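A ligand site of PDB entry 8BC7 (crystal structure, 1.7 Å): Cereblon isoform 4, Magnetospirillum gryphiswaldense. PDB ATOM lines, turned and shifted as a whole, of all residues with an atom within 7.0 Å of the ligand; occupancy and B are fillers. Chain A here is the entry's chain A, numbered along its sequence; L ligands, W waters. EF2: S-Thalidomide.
OH of Tyr 101 lies within hydrogen-bond range of O05 of the ligand. The backbone carbonyl oxygen (O) of Phe 77 is in hydrogen-bond range of a nitrogen (N03) of the ligand (2.9 Å). ND2 of Asn 50 sits at hydrogen-bond distance from O18 of the ligand, at 2.9 Å. An oxygen (O05) of the ligand lies within hydrogen-bond range of the backbone NH (N) of Trp 79 (3.1 Å).
The side-chain amide oxygen (OD1) of Asn 50 lies within hydrogen-bond range of the backbone NH (N) of Ala 52 (3.0 Å). The side-chain amide oxygen (OD1) of Asn 50 sits at hydrogen-bond distance from the backbone NH (N) of Met 54 (3.1 Å). The indole nitrogen (NE1) of Trp 79 is in hydrogen-bond range of the backbone carbonyl oxygen (O) of Phe 49. O of Glu 76 lies within hydrogen-bond range of NE1 of Trp 85, at 2.8 Å. The backbone carbonyl oxygen (O) of Ser 74 sits at hydrogen-bond distance from the backbone NH (N) of Trp 85 (2.7 Å). The backbone carbonyl oxygen of Phe 80 sits at hydrogen-bond distance from the side-chain hydroxyl of Ser 78 (3.0 Å). OG of Ser 78 lies within hydrogen-bond range of O of Tyr 83 (2.9 Å). The backbone NH (N) of Glu 76 lies within hydrogen-bond range of the side-chain hydroxyl (OG) of Ser 74.
Merely in contact with the ligand: Pro 51, Glu 76, Ser 78, Trp 85 and Trp 99. Hydrophobic or aromatic side chains that line the ligand: Pro 51, Phe 77, Trp 79, Trp 85, Trp 99 and Tyr 101. Nine residues have an atom within 4 Å of the ligand: Asn 50, Pro 51, Glu 76, Phe 77, Ser 78, Trp 79, Trp 85, Trp 99 and Tyr 101. The nearest printed residue that does not touch the ligand is Phe 56 (4.4 Å).
Water W1 lies within hydrogen-bond range of the indole nitrogen (NE1) of Trp 99 (2.9 Å) and an oxygen (O18) of the ligand (3.1 Å).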
ATOM      1  N   VAL A  48     -14.654  -8.895 -21.563  1.00  0.00           N
ATOM      2  CA  VAL A  48     -15.461  -7.863 -22.266  1.00  0.00           C
ATOM      3  C   VAL A  48     -14.536  -6.684 -22.579  1.00  0.00           C
ATOM      4  O   VAL A  48     -13.483  -6.562 -21.924  1.00  0.00           O
ATOM      5  CB  VAL A  48     -16.659  -7.471 -21.375  1.00  0.00           C
ATOM      6  CG1 VAL A  48     -17.642  -8.644 -21.265  1.00  0.00           C
ATOM      7  CG2 VAL A  48     -16.236  -6.987 -20.006  1.00  0.00           C
ATOM      8  N   PHE A  49     -14.890  -5.832 -23.519  1.00  0.00           N
ATOM      9  CA  PHE A  49     -14.186  -4.551 -23.705  1.00  0.00           C
ATOM     10  C   PHE A  49     -15.215  -3.414 -23.723  1.00  0.00           C
ATOM     11  O   PHE A  49     -16.374  -3.605 -24.229  1.00  0.00           O
ATOM     12  CB  PHE A  49     -13.265  -4.588 -24.929  1.00  0.00           C
ATOM     13  CG  PHE A  49     -13.939  -4.689 -26.242  1.00  0.00           C
ATOM     14  CD1 PHE A  49     -14.311  -5.917 -26.770  1.00  0.00           C
ATOM     15  CD2 PHE A  49     -14.195  -3.534 -26.991  1.00  0.00           C
ATOM     16  CE1 PHE A  49     -14.892  -5.986 -28.027  1.00  0.00           C
ATOM     17  CE2 PHE A  49     -14.729  -3.615 -28.281  1.00  0.00           C
ATOM     18  CZ  PHE A  49     -15.098  -4.846 -28.784  1.00  0.00           C
ATOM     19  N   ASN A  50     -14.800  -2.270 -23.208  1.00  0.00           N
ATOM     20  CA  ASN A  50     -15.608  -1.040 -23.287  1.00  0.00           C
ATOM     21  C   ASN A  50     -15.331  -0.240 -24.567  1.00  0.00           C
ATOM     22  O   ASN A  50     -14.526  -0.582 -25.457  1.00  0.00           O
ATOM     23  CB  ASN A  50     -15.416  -0.313 -21.957  1.00  0.00           C
ATOM     24  CG  ASN A  50     -14.127   0.459 -21.826  1.00  0.00           C
ATOM     25  OD1 ASN A  50     -13.317   0.507 -22.768  1.00  0.00           O
ATOM     26  ND2 ASN A  50     -13.964   1.074 -20.678  1.00  0.00           N
ATOM     27  N   PRO A  51     -16.072   0.859 -24.804  1.00  0.00           N
ATOM     28  CA  PRO A  51     -15.859   1.660 -26.002  1.00  0.00           C
ATOM     29  C   PRO A  51     -14.474   2.329 -26.107  1.00  0.00           C
ATOM     30  O   PRO A  51     -14.159   2.688 -27.173  1.00  0.00           O
ATOM     31  CB  PRO A  51     -16.968   2.718 -25.943  1.00  0.00           C
ATOM     32  CG  PRO A  51     -18.053   2.078 -25.078  1.00  0.00           C
ATOM     33  CD  PRO A  51     -17.268   1.298 -24.045  1.00  0.00           C
ATOM     34  N   ALA A  52     -13.731   2.452 -25.024  1.00  0.00           N
ATOM     35  CA  ALA A  52     -12.349   2.983 -25.006  1.00  0.00           C
ATOM     36  C   ALA A  52     -11.319   1.843 -25.246  1.00  0.00           C
ATOM     37  O   ALA A  52     -10.100   2.112 -25.155  1.00  0.00           O
ATOM     38  CB  ALA A  52     -12.088   3.678 -23.710  1.00  0.00           C
ATOM     39  N   MET A  54     -10.666  -0.831 -23.530  1.00  0.00           N
ATOM     40  CA  MET A  54     -10.121  -1.499 -22.332  1.00  0.00           C
ATOM     41  C   MET A  54     -10.733  -2.891 -22.201  1.00  0.00           C
ATOM     42  O   MET A  54     -11.992  -2.982 -22.242  1.00  0.00           O
ATOM     43  CB  MET A  54     -10.476  -0.680 -21.107  1.00  0.00           C
ATOM     44  CG  MET A  54      -9.910   0.686 -21.144  1.00  0.00           C
ATOM     45  SD  MET A  54      -9.972   1.336 -19.520  1.00  0.00           S
ATOM     46  CE  MET A  54      -9.107   0.048 -18.614  1.00  0.00           C
ATOM     47  N   PHE A  56     -11.587  -6.100 -19.821  1.00  0.00           N
ATOM     48  CA  PHE A  56     -11.800  -6.459 -18.387  1.00  0.00           C
ATOM     49  C   PHE A  56     -12.129  -7.940 -18.285  1.00  0.00           C
ATOM     50  O   PHE A  56     -12.969  -8.460 -19.073  1.00  0.00           O
ATOM     51  CB  PHE A  56     -12.966  -5.664 -17.791  1.00  0.00           C
ATOM     52  CG  PHE A  56     -12.814  -4.161 -17.818  1.00  0.00           C
ATOM     53  CD1 PHE A  56     -12.012  -3.492 -16.915  1.00  0.00           C
ATOM     54  CD2 PHE A  56     -13.372  -3.429 -18.840  1.00  0.00           C
ATOM     55  CE1 PHE A  56     -11.880  -2.117 -16.969  1.00  0.00           C
ATOM     56  CE2 PHE A  56     -13.239  -2.048 -18.864  1.00  0.00           C
ATOM     57  CZ  PHE A  56     -12.524  -1.395 -17.911  1.00  0.00           C
ATOM     58  N   SER A  74     -27.546   3.215 -16.553  1.00  0.00           N
ATOM     59  CA  SER A  74     -27.531   3.390 -18.024  1.00  0.00           C
ATOM     60  C   SER A  74     -27.618   2.012 -18.690  1.00  0.00           C
ATOM     61  O   SER A  74     -26.987   1.100 -18.199  1.00  0.00           O
ATOM     62  CB  SER A  74     -26.316   4.184 -18.499  1.00  0.00           C
ATOM     63  OG  SER A  74     -26.335   4.220 -19.923  1.00  0.00           O
ATOM     64  N   GLY A  75     -28.363   1.858 -19.760  1.00  0.00           N
ATOM     65  CA  GLY A  75     -28.393   0.638 -20.610  1.00  0.00           C
ATOM     66  C   GLY A  75     -27.356   0.651 -21.747  1.00  0.00           C
ATOM     67  O   GLY A  75     -27.135  -0.380 -22.358  1.00  0.00           O
ATOM     68  N   GLU A  76     -26.724   1.788 -21.997  1.00  0.00           N
ATOM     69  CA  GLU A  76     -25.782   2.000 -23.142  1.00  0.00           C
ATOM     70  C   GLU A  76     -24.600   1.037 -23.023  1.00  0.00           C
ATOM     71  O   GLU A  76     -24.014   0.967 -21.976  1.00  0.00           O
ATOM     72  CB  GLU A  76     -25.206   3.424 -23.140  1.00  0.00           C
ATOM     73  CG  GLU A  76     -26.235   4.443 -23.552  1.00  0.00           C
ATOM     74  CD  GLU A  76     -25.665   5.841 -23.772  1.00  0.00           C
ATOM     75  OE1 GLU A  76     -24.917   6.287 -22.880  1.00  0.00           O
ATOM     76  OE2 GLU A  76     -25.943   6.448 -24.857  1.00  0.00           O
ATOM     77  N   PHE A  77     -24.336   0.229 -24.054  1.00  0.00           N
ATOM     78  CA  PHE A  77     -23.110  -0.605 -24.169  1.00  0.00           C
ATOM     79  C   PHE A  77     -23.129  -1.710 -23.106  1.00  0.00           C
ATOM     80  O   PHE A  77     -22.059  -2.265 -22.820  1.00  0.00           O
ATOM     81  CB  PHE A  77     -21.846   0.236 -23.963  1.00  0.00           C
ATOM     82  CG  PHE A  77     -21.690   1.453 -24.850  1.00  0.00           C
ATOM     83  CD1 PHE A  77     -21.610   1.316 -26.213  1.00  0.00           C
ATOM     84  CD2 PHE A  77     -21.622   2.725 -24.300  1.00  0.00           C
ATOM     85  CE1 PHE A  77     -21.488   2.435 -27.043  1.00  0.00           C
ATOM     86  CE2 PHE A  77     -21.503   3.835 -25.117  1.00  0.00           C
ATOM     87  CZ  PHE A  77     -21.407   3.690 -26.484  1.00  0.00           C
ATOM     88  N   SER A  78     -24.267  -2.013 -22.459  1.00  0.00           N
ATOM     89  CA  SER A  78     -24.339  -3.073 -21.454  1.00  0.00           C
ATOM     90  C   SER A  78     -23.902  -4.392 -22.068  1.00  0.00           C
ATOM     91  O   SER A  78     -24.432  -4.772 -23.090  1.00  0.00           O
ATOM     92  CB  SER A  78     -25.728  -3.246 -20.839  1.00  0.00           C
ATOM     93  OG  SER A  78     -25.662  -4.216 -19.826  1.00  0.00           O
ATOM     94  N   TRP A  79     -22.959  -5.050 -21.394  1.00  0.00           N
ATOM     95  CA  TRP A  79     -22.457  -6.390 -21.761  1.00  0.00           C
ATOM     96  C   TRP A  79     -23.508  -7.450 -21.446  1.00  0.00           C
ATOM     97  O   TRP A  79     -23.366  -8.538 -21.939  1.00  0.00           O
ATOM     98  CB  TRP A  79     -21.161  -6.663 -20.993  1.00  0.00           C
ATOM     99  CG  TRP A  79     -20.047  -5.752 -21.403  1.00  0.00           C
ATOM    100  CD1 TRP A  79     -19.608  -5.443 -22.656  1.00  0.00           C
ATOM    101  CD2 TRP A  79     -19.188  -5.069 -20.496  1.00  0.00           C
ATOM    102  NE1 TRP A  79     -18.558  -4.563 -22.576  1.00  0.00           N
ATOM    103  CE2 TRP A  79     -18.262  -4.330 -21.258  1.00  0.00           C
ATOM    104  CE3 TRP A  79     -19.138  -4.997 -19.107  1.00  0.00           C
ATOM    105  CZ2 TRP A  79     -17.309  -3.512 -20.665  1.00  0.00           C
ATOM    106  CZ3 TRP A  79     -18.191  -4.207 -18.525  1.00  0.00           C
ATOM    107  CH2 TRP A  79     -17.287  -3.480 -19.290  1.00  0.00           C
ATOM    108  N   PHE A  80     -24.506  -7.161 -20.610  1.00  0.00           N
ATOM    109  CA  PHE A  80     -25.472  -8.181 -20.158  1.00  0.00           C
ATOM    110  C   PHE A  80     -26.860  -7.753 -20.621  1.00  0.00           C
ATOM    111  O   PHE A  80     -27.347  -6.701 -20.173  1.00  0.00           O
ATOM    112  CB  PHE A  80     -25.362  -8.376 -18.658  1.00  0.00           C
ATOM    113  CG  PHE A  80     -23.997  -8.807 -18.193  1.00  0.00           C
ATOM    114  CD1 PHE A  80     -23.594 -10.134 -18.314  1.00  0.00           C
ATOM    115  CD2 PHE A  80     -23.088  -7.887 -17.747  1.00  0.00           C
ATOM    116  CE1 PHE A  80     -22.358 -10.544 -17.843  1.00  0.00           C
ATOM    117  CE2 PHE A  80     -21.828  -8.311 -17.289  1.00  0.00           C
ATOM    118  CZ  PHE A  80     -21.479  -9.642 -17.354  1.00  0.00           C
ATOM    119  N   TYR A  83     -29.930  -5.580 -18.798  1.00  0.00           N
ATOM    120  CA  TYR A  83     -29.509  -4.930 -17.560  1.00  0.00           C
ATOM    121  C   TYR A  83     -28.978  -3.537 -17.851  1.00  0.00           C
ATOM    122  O   TYR A  83     -28.315  -3.317 -18.915  1.00  0.00           O
ATOM    123  CB  TYR A  83     -28.418  -5.730 -16.849  1.00  0.00           C
ATOM    124  CG  TYR A  83     -28.897  -7.067 -16.358  1.00  0.00           C
ATOM    125  CD1 TYR A  83     -29.474  -7.217 -15.113  1.00  0.00           C
ATOM    126  CD2 TYR A  83     -28.728  -8.197 -17.138  1.00  0.00           C
ATOM    127  CE1 TYR A  83     -29.915  -8.443 -14.661  1.00  0.00           C
ATOM    128  CE2 TYR A  83     -29.191  -9.440 -16.719  1.00  0.00           C
ATOM    129  CZ  TYR A  83     -29.763  -9.561 -15.462  1.00  0.00           C
ATOM    130  OH  TYR A  83     -30.187 -10.777 -15.061  1.00  0.00           O
ATOM    131  N   TRP A  85     -26.561  -0.442 -15.995  1.00  0.00           N
ATOM    132  CA  TRP A  85     -25.381  -0.452 -15.095  1.00  0.00           C
ATOM    133  C   TRP A  85     -25.217   0.868 -14.384  1.00  0.00           C
ATOM    134  O   TRP A  85     -25.535   1.934 -14.964  1.00  0.00           O
ATOM    135  CB  TRP A  85     -24.117  -0.877 -15.832  1.00  0.00           C
ATOM    136  CG  TRP A  85     -23.838  -0.095 -17.081  1.00  0.00           C
ATOM    137  CD1 TRP A  85     -24.160  -0.448 -18.346  1.00  0.00           C
ATOM    138  CD2 TRP A  85     -23.167   1.183 -17.156  1.00  0.00           C
ATOM    139  NE1 TRP A  85     -23.800   0.551 -19.199  1.00  0.00           N
ATOM    140  CE2 TRP A  85     -23.198   1.570 -18.499  1.00  0.00           C
ATOM    141  CE3 TRP A  85     -22.571   2.025 -16.196  1.00  0.00           C
ATOM    142  CZ2 TRP A  85     -22.668   2.781 -18.934  1.00  0.00           C
ATOM    143  CZ3 TRP A  85     -22.040   3.228 -16.637  1.00  0.00           C
ATOM    144  CH2 TRP A  85     -22.048   3.576 -17.992  1.00  0.00           C
ATOM    145  N   THR A  86     -24.570   0.785 -13.196  1.00  0.00           N
ATOM    146  CA  THR A  86     -24.014   1.929 -12.457  1.00  0.00           C
ATOM    147  C   THR A  86     -22.569   1.559 -12.152  1.00  0.00           C
ATOM    148  O   THR A  86     -22.305   0.404 -11.777  1.00  0.00           O
ATOM    149  CB  THR A  86     -24.852   2.323 -11.241  1.00  0.00           C
ATOM    150  OG1 THR A  86     -24.825   1.179 -10.409  1.00  0.00           O
ATOM    151  CG2 THR A  86     -26.283   2.654 -11.596  1.00  0.00           C
ATOM    152  N   ILE A  87     -21.726   2.553 -12.148  1.00  0.00           N
ATOM    153  CA  ILE A  87     -20.301   2.428 -11.728  1.00  0.00           C
ATOM    154  C   ILE A  87     -20.259   2.101 -10.234  1.00  0.00           C
ATOM    155  O   ILE A  87     -20.969   2.760  -9.384  1.00  0.00           O
ATOM    156  CB  ILE A  87     -19.569   3.718 -12.074  1.00  0.00           C
ATOM    157  CG1 ILE A  87     -19.430   3.838 -13.610  1.00  0.00           C
ATOM    158  CG2 ILE A  87     -18.210   3.702 -11.384  1.00  0.00           C
ATOM    159  CD1 ILE A  87     -19.152   5.217 -14.138  1.00  0.00           C
ATOM    160  N   HIS A  96     -12.021   2.226  -8.866  1.00  0.00           N
ATOM    161  CA  HIS A  96     -13.094   1.626  -9.689  1.00  0.00           C
ATOM    162  C   HIS A  96     -13.060   0.091  -9.623  1.00  0.00           C
ATOM    163  O   HIS A  96     -12.035  -0.483 -10.118  1.00  0.00           O
ATOM    164  CB  HIS A  96     -12.945   2.134 -11.142  1.00  0.00           C
ATOM    165  CG  HIS A  96     -14.008   1.554 -11.977  1.00  0.00           C
ATOM    166  ND1 HIS A  96     -13.800   1.222 -13.315  1.00  0.00           N
ATOM    167  CD2 HIS A  96     -15.272   1.131 -11.663  1.00  0.00           C
ATOM    168  CE1 HIS A  96     -14.921   0.748 -13.801  1.00  0.00           C
ATOM    169  NE2 HIS A  96     -15.845   0.677 -12.819  1.00  0.00           N
ATOM    170  N   GLY A  98     -15.845  -2.072 -10.490  1.00  0.00           N
ATOM    171  CA  GLY A  98     -16.721  -2.725 -11.465  1.00  0.00           C
ATOM    172  C   GLY A  98     -18.028  -1.965 -11.637  1.00  0.00           C
ATOM    173  O   GLY A  98     -18.020  -0.709 -11.613  1.00  0.00           O
ATOM    174  N   TRP A  99     -19.090  -2.727 -11.753  1.00  0.00           N
ATOM    175  CA  TRP A  99     -20.459  -2.157 -12.009  1.00  0.00           C
ATOM    176  C   TRP A  99     -21.499  -2.936 -11.217  1.00  0.00           C
ATOM    177  O   TRP A  99     -21.337  -4.156 -11.050  1.00  0.00           O
ATOM    178  CB  TRP A  99     -20.753  -2.131 -13.508  1.00  0.00           C
ATOM    179  CG  TRP A  99     -19.671  -1.461 -14.311  1.00  0.00           C
ATOM    180  CD1 TRP A  99     -19.639  -0.148 -14.672  1.00  0.00           C
ATOM    181  CD2 TRP A  99     -18.432  -2.033 -14.799  1.00  0.00           C
ATOM    182  NE1 TRP A  99     -18.484   0.132 -15.373  1.00  0.00           N
ATOM    183  CE2 TRP A  99     -17.741  -1.014 -15.491  1.00  0.00           C
ATOM    184  CE3 TRP A  99     -17.856  -3.307 -14.793  1.00  0.00           C
ATOM    185  CZ2 TRP A  99     -16.481  -1.211 -16.081  1.00  0.00           C
ATOM    186  CZ3 TRP A  99     -16.613  -3.520 -15.379  1.00  0.00           C
ATOM    187  CH2 TRP A  99     -15.929  -2.474 -16.021  1.00  0.00           C
ATOM    188  N   TYR A 101     -25.442  -4.075 -11.791  1.00  0.00           N
ATOM    189  CA  TYR A 101     -26.409  -4.284 -12.879  1.00  0.00           C
ATOM    190  C   TYR A 101     -27.796  -4.400 -12.261  1.00  0.00           C
ATOM    191  O   TYR A 101     -27.915  -5.051 -11.213  1.00  0.00           O
ATOM    192  CB  TYR A 101     -26.012  -5.535 -13.661  1.00  0.00           C
ATOM    193  CG  TYR A 101     -24.807  -5.326 -14.544  1.00  0.00           C
ATOM    194  CD1 TYR A 101     -24.916  -4.740 -15.780  1.00  0.00           C
ATOM    195  CD2 TYR A 101     -23.529  -5.597 -14.043  1.00  0.00           C
ATOM    196  CE1 TYR A 101     -23.800  -4.562 -16.606  1.00  0.00           C
ATOM    197  CE2 TYR A 101     -22.410  -5.390 -14.840  1.00  0.00           C
ATOM    198  CZ  TYR A 101     -22.536  -4.833 -16.108  1.00  0.00           C
ATOM    199  OH  TYR A 101     -21.387  -4.621 -16.871  1.00  0.00           O
HETATM  200  O01 EF2 L   1     -19.052  -0.609 -21.686  1.00  0.00           O
HETATM  201  C02 EF2 L   1     -19.483  -0.849 -20.599  1.00  0.00           C
HETATM  202  N03 EF2 L   1     -20.465  -1.824 -20.463  1.00  0.00           N
HETATM  203  C04 EF2 L   1     -21.039  -2.255 -19.280  1.00  0.00           C
HETATM  204  O05 EF2 L   1     -21.752  -3.247 -19.250  1.00  0.00           O
HETATM  205  C06 EF2 L   1     -20.613  -1.532 -18.063  1.00  0.00           C
HETATM  206  C07 EF2 L   1     -20.117  -0.103 -18.303  1.00  0.00           C
HETATM  207  C08 EF2 L   1     -19.038  -0.080 -19.357  1.00  0.00           C
HETATM  208  N09 EF2 L   1     -18.593   1.255 -19.737  1.00  0.00           N
HETATM  209  C11 EF2 L   1     -17.329   5.156 -21.938  1.00  0.00           C
HETATM  210  C12 EF2 L   1     -18.433   4.313 -21.783  1.00  0.00           C
HETATM  211  C13 EF2 L   1     -18.278   3.217 -20.972  1.00  0.00           C
HETATM  212  C14 EF2 L   1     -17.102   2.948 -20.300  1.00  0.00           C
HETATM  213  O16 EF2 L   1     -20.338   1.988 -21.119  1.00  0.00           O
HETATM  214  O18 EF2 L   1     -16.456   0.909 -19.155  1.00  0.00           O
HETATM  215  C19 EF2 L   1     -15.994   3.750 -20.483  1.00  0.00           C
HETATM  216  C20 EF2 L   1     -16.135   4.878 -21.287  1.00  0.00           C
HETATM  217  C3  EF2 L   1     -17.269   1.671 -19.565  1.00  0.00           C
HETATM  218  C4  EF2 L   1     -19.238   2.126 -20.650  1.00  0.00           C
HETATM  219  O   HOH W   1     -17.141   2.414 -16.529  1.00  0.00           O
